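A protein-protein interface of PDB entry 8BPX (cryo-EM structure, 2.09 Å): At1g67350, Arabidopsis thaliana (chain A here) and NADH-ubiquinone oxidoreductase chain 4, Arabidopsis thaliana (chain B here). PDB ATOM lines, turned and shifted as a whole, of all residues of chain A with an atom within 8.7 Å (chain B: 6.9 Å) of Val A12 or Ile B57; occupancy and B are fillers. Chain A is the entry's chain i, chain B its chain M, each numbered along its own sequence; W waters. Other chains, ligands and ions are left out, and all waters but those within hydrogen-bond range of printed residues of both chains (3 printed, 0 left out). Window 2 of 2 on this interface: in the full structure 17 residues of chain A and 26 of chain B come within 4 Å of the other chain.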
ATOM      1  N   MET A   5      22.618  -5.624  26.745  1.00  0.00           N
ATOM      2  CA  MET A   5      21.994  -6.929  26.806  1.00  0.00           C
ATOM      3  C   MET A   5      20.484  -6.810  26.994  1.00  0.00           C
ATOM      4  O   MET A   5      19.809  -7.532  26.294  1.00  0.00           O
ATOM      5  CB  MET A   5      22.704  -7.815  27.827  1.00  0.00           C
ATOM      6  CG  MET A   5      23.040  -9.183  27.272  1.00  0.00           C
ATOM      7  SD  MET A   5      24.316  -9.149  25.970  1.00  0.00           S
ATOM      8  CE  MET A   5      24.263 -10.857  25.456  1.00  0.00           C
ATOM      9  N   GLU A   6      19.979  -5.899  27.821  1.00  0.00           N
ATOM     10  CA  GLU A   6      18.518  -5.879  28.025  1.00  0.00           C
ATOM     11  C   GLU A   6      17.866  -5.566  26.670  1.00  0.00           C
ATOM     12  O   GLU A   6      16.951  -6.294  26.300  1.00  0.00           O
ATOM     13  CB  GLU A   6      18.103  -4.988  29.197  1.00  0.00           C
ATOM     14  CG  GLU A   6      16.601  -4.909  29.375  1.00  0.00           C
ATOM     15  CD  GLU A   6      16.101  -3.650  30.061  1.00  0.00           C
ATOM     16  OE1 GLU A   6      16.879  -2.677  30.149  1.00  0.00           O
ATOM     17  OE2 GLU A   6      14.935  -3.644  30.501  1.00  0.00           O
ATOM     18  N   PHE A   7      18.415  -4.620  25.936  1.00  0.00           N
ATOM     19  CA  PHE A   7      17.903  -4.315  24.582  1.00  0.00           C
ATOM     20  C   PHE A   7      18.003  -5.597  23.746  1.00  0.00           C
ATOM     21  O   PHE A   7      17.077  -5.876  23.049  1.00  0.00           O
ATOM     22  CB  PHE A   7      18.625  -3.089  23.998  1.00  0.00           C
ATOM     23  CG  PHE A   7      18.454  -2.926  22.518  1.00  0.00           C
ATOM     24  CD1 PHE A   7      19.248  -3.634  21.631  1.00  0.00           C
ATOM     25  CD2 PHE A   7      17.467  -2.104  22.015  1.00  0.00           C
ATOM     26  CE1 PHE A   7      19.063  -3.506  20.269  1.00  0.00           C
ATOM     27  CE2 PHE A   7      17.288  -1.975  20.653  1.00  0.00           C
ATOM     28  CZ  PHE A   7      18.088  -2.671  19.783  1.00  0.00           C
ATOM     29  N   ALA A   8      19.144  -6.287  23.816  1.00  0.00           N
ATOM     30  CA  ALA A   8      19.305  -7.494  23.012  1.00  0.00           C
ATOM     31  C   ALA A   8      18.279  -8.562  23.391  1.00  0.00           C
ATOM     32  O   ALA A   8      17.736  -9.243  22.514  1.00  0.00           O
ATOM     33  CB  ALA A   8      20.728  -8.027  23.149  1.00  0.00           C
ATOM     34  N   GLU A   9      18.010  -8.723  24.691  1.00  0.00           N
ATOM     35  CA  GLU A   9      16.942  -9.619  25.135  1.00  0.00           C
ATOM     36  C   GLU A   9      15.633  -9.280  24.445  1.00  0.00           C
ATOM     37  O   GLU A   9      14.971 -10.149  23.860  1.00  0.00           O
ATOM     38  CB  GLU A   9      16.715  -9.531  26.648  1.00  0.00           C
ATOM     39  CG  GLU A   9      17.436 -10.476  27.600  1.00  0.00           C
ATOM     40  CD  GLU A   9      18.938 -10.429  27.567  1.00  0.00           C
ATOM     41  OE1 GLU A   9      19.516  -9.479  28.127  1.00  0.00           O
ATOM     42  OE2 GLU A   9      19.547 -11.384  27.074  1.00  0.00           O
ATOM     43  N   ASN A  10      15.248  -8.008  24.515  1.00  0.00           N
ATOM     44  CA  ASN A  10      13.968  -7.597  23.953  1.00  0.00           C
ATOM     45  C   ASN A  10      13.934  -7.793  22.444  1.00  0.00           C
ATOM     46  O   ASN A  10      12.926  -8.248  21.895  1.00  0.00           O
ATOM     47  CB  ASN A  10      13.677  -6.148  24.330  1.00  0.00           C
ATOM     48  CG  ASN A  10      13.318  -5.997  25.786  1.00  0.00           C
ATOM     49  OD1 ASN A  10      13.178  -6.986  26.503  1.00  0.00           O
ATOM     50  ND2 ASN A  10      13.166  -4.757  26.237  1.00  0.00           N
ATOM     51  N   LEU A  11      15.028  -7.464  21.760  1.00  0.00           N
ATOM     52  CA  LEU A  11      15.073  -7.620  20.310  1.00  0.00           C
ATOM     53  C   LEU A  11      14.939  -9.085  19.906  1.00  0.00           C
ATOM     54  O   LEU A  11      14.180  -9.424  18.988  1.00  0.00           O
ATOM     55  CB  LEU A  11      16.369  -7.016  19.773  1.00  0.00           C
ATOM     56  CG  LEU A  11      16.638  -7.095  18.275  1.00  0.00           C
ATOM     57  CD1 LEU A  11      15.410  -6.678  17.478  1.00  0.00           C
ATOM     58  CD2 LEU A  11      17.833  -6.246  17.922  1.00  0.00           C
ATOM     59  N   VAL A  12      15.642  -9.986  20.600  1.00  0.00           N
ATOM     60  CA  VAL A  12      15.606 -11.431  20.205  1.00  0.00           C
ATOM     61  C   VAL A  12      14.184 -11.988  20.394  1.00  0.00           C
ATOM     62  O   VAL A  12      13.712 -12.713  19.506  1.00  0.00           O
ATOM     63  CB  VAL A  12      16.666 -12.273  20.943  1.00  0.00           C
ATOM     64  CG1 VAL A  12      16.439 -13.765  20.763  1.00  0.00           C
ATOM     65  CG2 VAL A  12      18.084 -11.891  20.557  1.00  0.00           C
ATOM     66  N   LEU A  13      13.514 -11.626  21.494  1.00  0.00           N
ATOM     67  CA  LEU A  13      12.135 -12.109  21.757  1.00  0.00           C
ATOM     68  C   LEU A  13      11.168 -11.620  20.666  1.00  0.00           C
ATOM     69  O   LEU A  13      10.263 -12.381  20.306  1.00  0.00           O
ATOM     70  CB  LEU A  13      11.692 -11.663  23.154  1.00  0.00           C
ATOM     71  CG  LEU A  13      12.375 -12.347  24.334  1.00  0.00           C
ATOM     72  CD1 LEU A  13      12.086 -11.594  25.621  1.00  0.00           C
ATOM     73  CD2 LEU A  13      11.944 -13.798  24.456  1.00  0.00           C
ATOM     74  N   ARG A  14      11.364 -10.403  20.163  1.00  0.00           N
ATOM     75  CA  ARG A  14      10.535  -9.806  19.085  1.00  0.00           C
ATOM     76  C   ARG A  14      10.743 -10.559  17.759  1.00  0.00           C
ATOM     77  O   ARG A  14       9.815 -10.588  16.964  1.00  0.00           O
ATOM     78  CB  ARG A  14      10.855  -8.313  18.930  1.00  0.00           C
ATOM     79  CG  ARG A  14       9.853  -7.380  19.589  1.00  0.00           C
ATOM     80  CD  ARG A  14      10.542  -6.268  20.358  1.00  0.00           C
ATOM     81  NE  ARG A  14      11.581  -5.609  19.577  1.00  0.00           N
ATOM     82  CZ  ARG A  14      12.598  -4.929  20.093  1.00  0.00           C
ATOM     83  NH1 ARG A  14      12.724  -4.813  21.402  1.00  0.00           N
ATOM     84  NH2 ARG A  14      13.487  -4.365  19.296  1.00  0.00           N
ATOM     85  N   LEU A  15      11.918 -11.160  17.564  1.00  0.00           N
ATOM     86  CA  LEU A  15      12.254 -11.888  16.313  1.00  0.00           C
ATOM     87  C   LEU A  15      11.532 -13.234  16.250  1.00  0.00           C
ATOM     88  O   LEU A  15      11.358 -13.752  15.153  1.00  0.00           O
ATOM     89  CB  LEU A  15      13.762 -12.080  16.242  1.00  0.00           C
ATOM     90  CG  LEU A  15      14.576 -10.808  16.016  1.00  0.00           C
ATOM     91  CD1 LEU A  15      16.061 -11.083  16.173  1.00  0.00           C
ATOM     92  CD2 LEU A  15      14.283 -10.209  14.655  1.00  0.00           C
ATOM     93  N   MET A  16      11.170 -13.769  17.403  1.00  0.00           N
ATOM     94  CA  MET A  16      10.896 -15.217  17.564  1.00  0.00           C
ATOM     95  C   MET A  16       9.424 -15.446  17.225  1.00  0.00           C
ATOM     96  O   MET A  16       8.666 -14.480  17.243  1.00  0.00           O
ATOM     97  CB  MET A  16      11.229 -15.678  18.985  1.00  0.00           C
ATOM     98  CG  MET A  16      12.706 -15.861  19.231  1.00  0.00           C
ATOM     99  SD  MET A  16      13.062 -16.425  20.908  1.00  0.00           S
ATOM    100  CE  MET A  16      14.384 -17.595  20.615  1.00  0.00           C
ATOM    101  N   GLU A  17       9.071 -16.658  16.817  1.00  0.00           N
ATOM    102  CA  GLU A  17       7.637 -16.994  16.631  1.00  0.00           C
ATOM    103  C   GLU A  17       6.942 -16.940  17.992  1.00  0.00           C
ATOM    104  O   GLU A  17       7.566 -17.344  18.993  1.00  0.00           O
ATOM    105  CB  GLU A  17       7.486 -18.379  16.019  1.00  0.00           C
ATOM    106  CG  GLU A  17       8.032 -18.492  14.613  1.00  0.00           C
ATOM    107  CD  GLU A  17       7.765 -19.847  13.984  1.00  0.00           C
ATOM    108  OE1 GLU A  17       6.736 -19.979  13.308  1.00  0.00           O
ATOM    109  OE2 GLU A  17       8.573 -20.767  14.196  1.00  0.00           O
ATOM    110  N   SER B  52      21.549 -16.723   7.682  1.00  0.00           N
ATOM    111  CA  SER B  52      21.435 -18.006   8.375  1.00  0.00           C
ATOM    112  C   SER B  52      21.812 -17.880   9.851  1.00  0.00           C
ATOM    113  O   SER B  52      21.206 -18.532  10.712  1.00  0.00           O
ATOM    114  CB  SER B  52      22.301 -19.057   7.682  1.00  0.00           C
ATOM    115  OG  SER B  52      23.636 -19.011   8.145  1.00  0.00           O
ATOM    116  N   LEU B  53      22.817 -17.059  10.159  1.00  0.00           N
ATOM    117  CA  LEU B  53      23.166 -16.826  11.560  1.00  0.00           C
ATOM    118  C   LEU B  53      21.993 -16.217  12.323  1.00  0.00           C
ATOM    119  O   LEU B  53      21.680 -16.631  13.449  1.00  0.00           O
ATOM    120  CB  LEU B  53      24.395 -15.922  11.652  1.00  0.00           C
ATOM    121  CG  LEU B  53      25.747 -16.561  11.325  1.00  0.00           C
ATOM    122  CD1 LEU B  53      26.890 -15.703  11.842  1.00  0.00           C
ATOM    123  CD2 LEU B  53      25.837 -17.972  11.890  1.00  0.00           C
ATOM    124  N   VAL B  54      21.316 -15.246  11.710  1.00  0.00           N
ATOM    125  CA  VAL B  54      20.126 -14.675  12.335  1.00  0.00           C
ATOM    126  C   VAL B  54      19.080 -15.758  12.565  1.00  0.00           C
ATOM    127  O   VAL B  54      18.476 -15.844  13.642  1.00  0.00           O
ATOM    128  CB  VAL B  54      19.566 -13.522  11.487  1.00  0.00           C
ATOM    129  CG1 VAL B  54      18.276 -13.010  12.099  1.00  0.00           C
ATOM    130  CG2 VAL B  54      20.588 -12.407  11.373  1.00  0.00           C
ATOM    131  N   LEU B  55      18.856 -16.607  11.556  1.00  0.00           N
ATOM    132  CA  LEU B  55      17.907 -17.707  11.716  1.00  0.00           C
ATOM    133  C   LEU B  55      18.266 -18.581  12.911  1.00  0.00           C
ATOM    134  O   LEU B  55      17.381 -19.062  13.627  1.00  0.00           O
ATOM    135  CB  LEU B  55      17.845 -18.549  10.444  1.00  0.00           C
ATOM    136  CG  LEU B  55      17.067 -17.954   9.270  1.00  0.00           C
ATOM    137  CD1 LEU B  55      16.659 -19.049   8.307  1.00  0.00           C
ATOM    138  CD2 LEU B  55      15.851 -17.186   9.758  1.00  0.00           C
ATOM    139  N   TRP B  56      19.561 -18.797  13.141  1.00  0.00           N
ATOM    140  CA  TRP B  56      19.975 -19.477  14.366  1.00  0.00           C
ATOM    141  C   TRP B  56      19.529 -18.695  15.596  1.00  0.00           C
ATOM    142  O   TRP B  56      19.046 -19.280  16.572  1.00  0.00           O
ATOM    143  CB  TRP B  56      21.490 -19.683  14.386  1.00  0.00           C
ATOM    144  CG  TRP B  56      21.995 -20.499  15.555  1.00  0.00           C
ATOM    145  CD1 TRP B  56      21.247 -21.097  16.529  1.00  0.00           C
ATOM    146  CD2 TRP B  56      23.363 -20.796  15.870  1.00  0.00           C
ATOM    147  NE1 TRP B  56      22.059 -21.742  17.427  1.00  0.00           N
ATOM    148  CE2 TRP B  56      23.362 -21.579  17.041  1.00  0.00           C
ATOM    149  CE3 TRP B  56      24.584 -20.484  15.268  1.00  0.00           C
ATOM    150  CZ2 TRP B  56      24.535 -22.050  17.626  1.00  0.00           C
ATOM    151  CZ3 TRP B  56      25.748 -20.953  15.849  1.00  0.00           C
ATOM    152  CH2 TRP B  56      25.715 -21.729  17.016  1.00  0.00           C
ATOM    153  N   ILE B  57      19.594 -17.366  15.653  1.00  0.00           N
ATOM    154  CA  ILE B  57      19.233 -16.641  16.916  1.00  0.00           C
ATOM    155  C   ILE B  57      17.733 -16.771  17.250  1.00  0.00           C
ATOM    156  O   ILE B  57      17.420 -16.968  18.414  1.00  0.00           O
ATOM    157  CB  ILE B  57      19.707 -15.165  16.868  1.00  0.00           C
ATOM    158  CG1 ILE B  57      21.232 -15.069  16.792  1.00  0.00           C
ATOM    159  CG2 ILE B  57      19.160 -14.359  18.033  1.00  0.00           C
ATOM    160  CD1 ILE B  57      21.952 -15.923  17.799  1.00  0.00           C
ATOM    161  N   GLN B  58      16.854 -16.695  16.252  1.00  0.00           N
ATOM    162  CA  GLN B  58      15.396 -16.731  16.500  1.00  0.00           C
ATOM    163  C   GLN B  58      14.891 -18.169  16.740  1.00  0.00           C
ATOM    164  O   GLN B  58      13.691 -18.335  16.858  1.00  0.00           O
ATOM    165  CB  GLN B  58      14.638 -16.088  15.350  1.00  0.00           C
ATOM    166  CG  GLN B  58      14.987 -16.656  13.991  1.00  0.00           C
ATOM    167  CD  GLN B  58      14.362 -15.809  12.916  1.00  0.00           C
ATOM    168  OE1 GLN B  58      14.573 -14.603  12.864  1.00  0.00           O
ATOM    169  NE2 GLN B  58      13.578 -16.438  12.060  1.00  0.00           N
ATOM    170  N   PHE B  59      15.792 -19.139  16.829  1.00  0.00           N
ATOM    171  CA  PHE B  59      15.409 -20.562  16.942  1.00  0.00           C
ATOM    172  C   PHE B  59      15.012 -20.864  18.386  1.00  0.00           C
ATOM    173  O   PHE B  59      15.679 -20.444  19.311  1.00  0.00           O
ATOM    174  CB  PHE B  59      16.559 -21.482  16.537  1.00  0.00           C
ATOM    175  CG  PHE B  59      16.245 -22.955  16.549  1.00  0.00           C
ATOM    176  CD1 PHE B  59      15.654 -23.562  15.454  1.00  0.00           C
ATOM    177  CD2 PHE B  59      16.558 -23.737  17.649  1.00  0.00           C
ATOM    178  CE1 PHE B  59      15.385 -24.920  15.459  1.00  0.00           C
ATOM    179  CE2 PHE B  59      16.268 -25.089  17.660  1.00  0.00           C
ATOM    180  CZ  PHE B  59      15.687 -25.680  16.564  1.00  0.00           C
ATOM    181  N   ASP B  60      13.988 -21.680  18.513  1.00  0.00           N
ATOM    182  CA  ASP B  60      13.339 -22.011  19.781  1.00  0.00           C
ATOM    183  C   ASP B  60      13.678 -23.469  20.085  1.00  0.00           C
ATOM    184  O   ASP B  60      13.204 -24.380  19.400  1.00  0.00           O
ATOM    185  CB  ASP B  60      11.830 -21.767  19.691  1.00  0.00           C
ATOM    186  CG  ASP B  60      11.016 -22.606  20.675  1.00  0.00           C
ATOM    187  OD1 ASP B  60      11.544 -23.022  21.727  1.00  0.00           O
ATOM    188  OD2 ASP B  60       9.828 -22.849  20.384  1.00  0.00           O
ATOM    189  N   PHE B  68       9.590 -21.778  11.833  1.00  0.00           N
ATOM    190  CA  PHE B  68       9.631 -20.848  10.678  1.00  0.00           C
ATOM    191  C   PHE B  68       8.768 -21.499   9.612  1.00  0.00           C
ATOM    192  O   PHE B  68       8.899 -21.158   8.445  1.00  0.00           O
ATOM    193  CB  PHE B  68      11.078 -20.496  10.294  1.00  0.00           C
ATOM    194  CG  PHE B  68      11.947 -20.201  11.489  1.00  0.00           C
ATOM    195  CD1 PHE B  68      11.489 -19.384  12.512  1.00  0.00           C
ATOM    196  CD2 PHE B  68      13.208 -20.758  11.605  1.00  0.00           C
ATOM    197  CE1 PHE B  68      12.277 -19.132  13.622  1.00  0.00           C
ATOM    198  CE2 PHE B  68      13.995 -20.498  12.714  1.00  0.00           C
ATOM    199  CZ  PHE B  68      13.528 -19.686  13.718  1.00  0.00           C
ATOM    200  N   LEU B  91      18.915 -27.357  11.212  1.00  0.00           N
ATOM    201  CA  LEU B  91      19.341 -25.963  11.335  1.00  0.00           C
ATOM    202  C   LEU B  91      20.831 -25.797  11.036  1.00  0.00           C
ATOM    203  O   LEU B  91      21.228 -25.002  10.167  1.00  0.00           O
ATOM    204  CB  LEU B  91      19.001 -25.470  12.748  1.00  0.00           C
ATOM    205  CG  LEU B  91      19.055 -24.007  13.200  1.00  0.00           C
ATOM    206  CD1 LEU B  91      20.465 -23.603  13.562  1.00  0.00           C
ATOM    207  CD2 LEU B  91      18.475 -23.068  12.153  1.00  0.00           C
ATOM    208  N   ILE B  95      23.194 -23.763   8.179  1.00  0.00           N
ATOM    209  CA  ILE B  95      24.289 -22.863   8.536  1.00  0.00           C
ATOM    210  C   ILE B  95      25.595 -23.309   7.882  1.00  0.00           C
ATOM    211  O   ILE B  95      26.360 -22.484   7.371  1.00  0.00           O
ATOM    212  CB  ILE B  95      24.424 -22.755  10.067  1.00  0.00           C
ATOM    213  CG1 ILE B  95      23.344 -21.833  10.628  1.00  0.00           C
ATOM    214  CG2 ILE B  95      25.801 -22.242  10.455  1.00  0.00           C
ATOM    215  CD1 ILE B  95      23.183 -21.936  12.122  1.00  0.00           C
HETATM  216  O   HOH W   1      13.034 -12.642  12.798  1.00  0.00           O
HETATM  217  O   HOH W   2       6.337 -22.323  12.212  1.00  0.00           O
HETATM  218  O   HOH W   3      11.181 -18.650  17.382  1.00  0.00           O
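N of Phe B68 is in hydrogen-bond range of OE2 of Glu A17, 2.8 Å away.
Among the printed residues, pairs that only touch across the chains: Met A16 with Phe B59, Met A16 with Gln B58, Val A12 with Ile B57 and Met A16 with Ile B57.
Val A12 touches just one residue of chain B: Ile B57. Of the printed residues of chain B, Met A16 touches Ile B57 (3.8 Å), Gln B58 (3.6 Å) and Phe B59 (3.4 Å). Of the printed residues of chain B, Glu A17 touches Phe B68 (2.8 Å). Of chain A, only Val A12 and Met A16 come within 4 Å of Ile B57. Of the printed residues of chain A, Gln B58 touches Met A16 (3.6 Å). Printed residues of chain A within 4 Å of Phe B59: Met A16. Printed residues of chain A within 4 Å of Phe B68: Glu A17 (2.8 Å). The nearest residue of chain A that does not touch Ile B57 is Leu A15 (4.9 Å).
Of the 13 printed residues of chain A, 3 touch a printed residue of chain B. Printed residues of chain A that touch a printed residue of chain B: Val A12, Met A16 and Glu A17. Hydrophobic or aromatic side chains of chain A within 4 Å of the printed part of chain B: Val A12 and Met A16. Among the printed residues, 5 pairs touch across the chains. Among the printed residues, no Asp or Glu carboxylate lies within 4 Å of a Lys or Arg side-chain nitrogen of the other chain.
Water W1 bridges OE1 of Gln B58 (2.5 Å) and O of Leu A15 (3.1 Å). Water W3 bridges the backbone carbonyl oxygen of Gln B58 (2.6 Å) and the backbone NH of Glu A17 (3.0 Å). Water W2 lies within hydrogen-bond range of the side-chain carboxylate (OE1) of Glu A17 (2.6 Å) and the backbone NH (N) of Phe B68 (3.3 Å).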
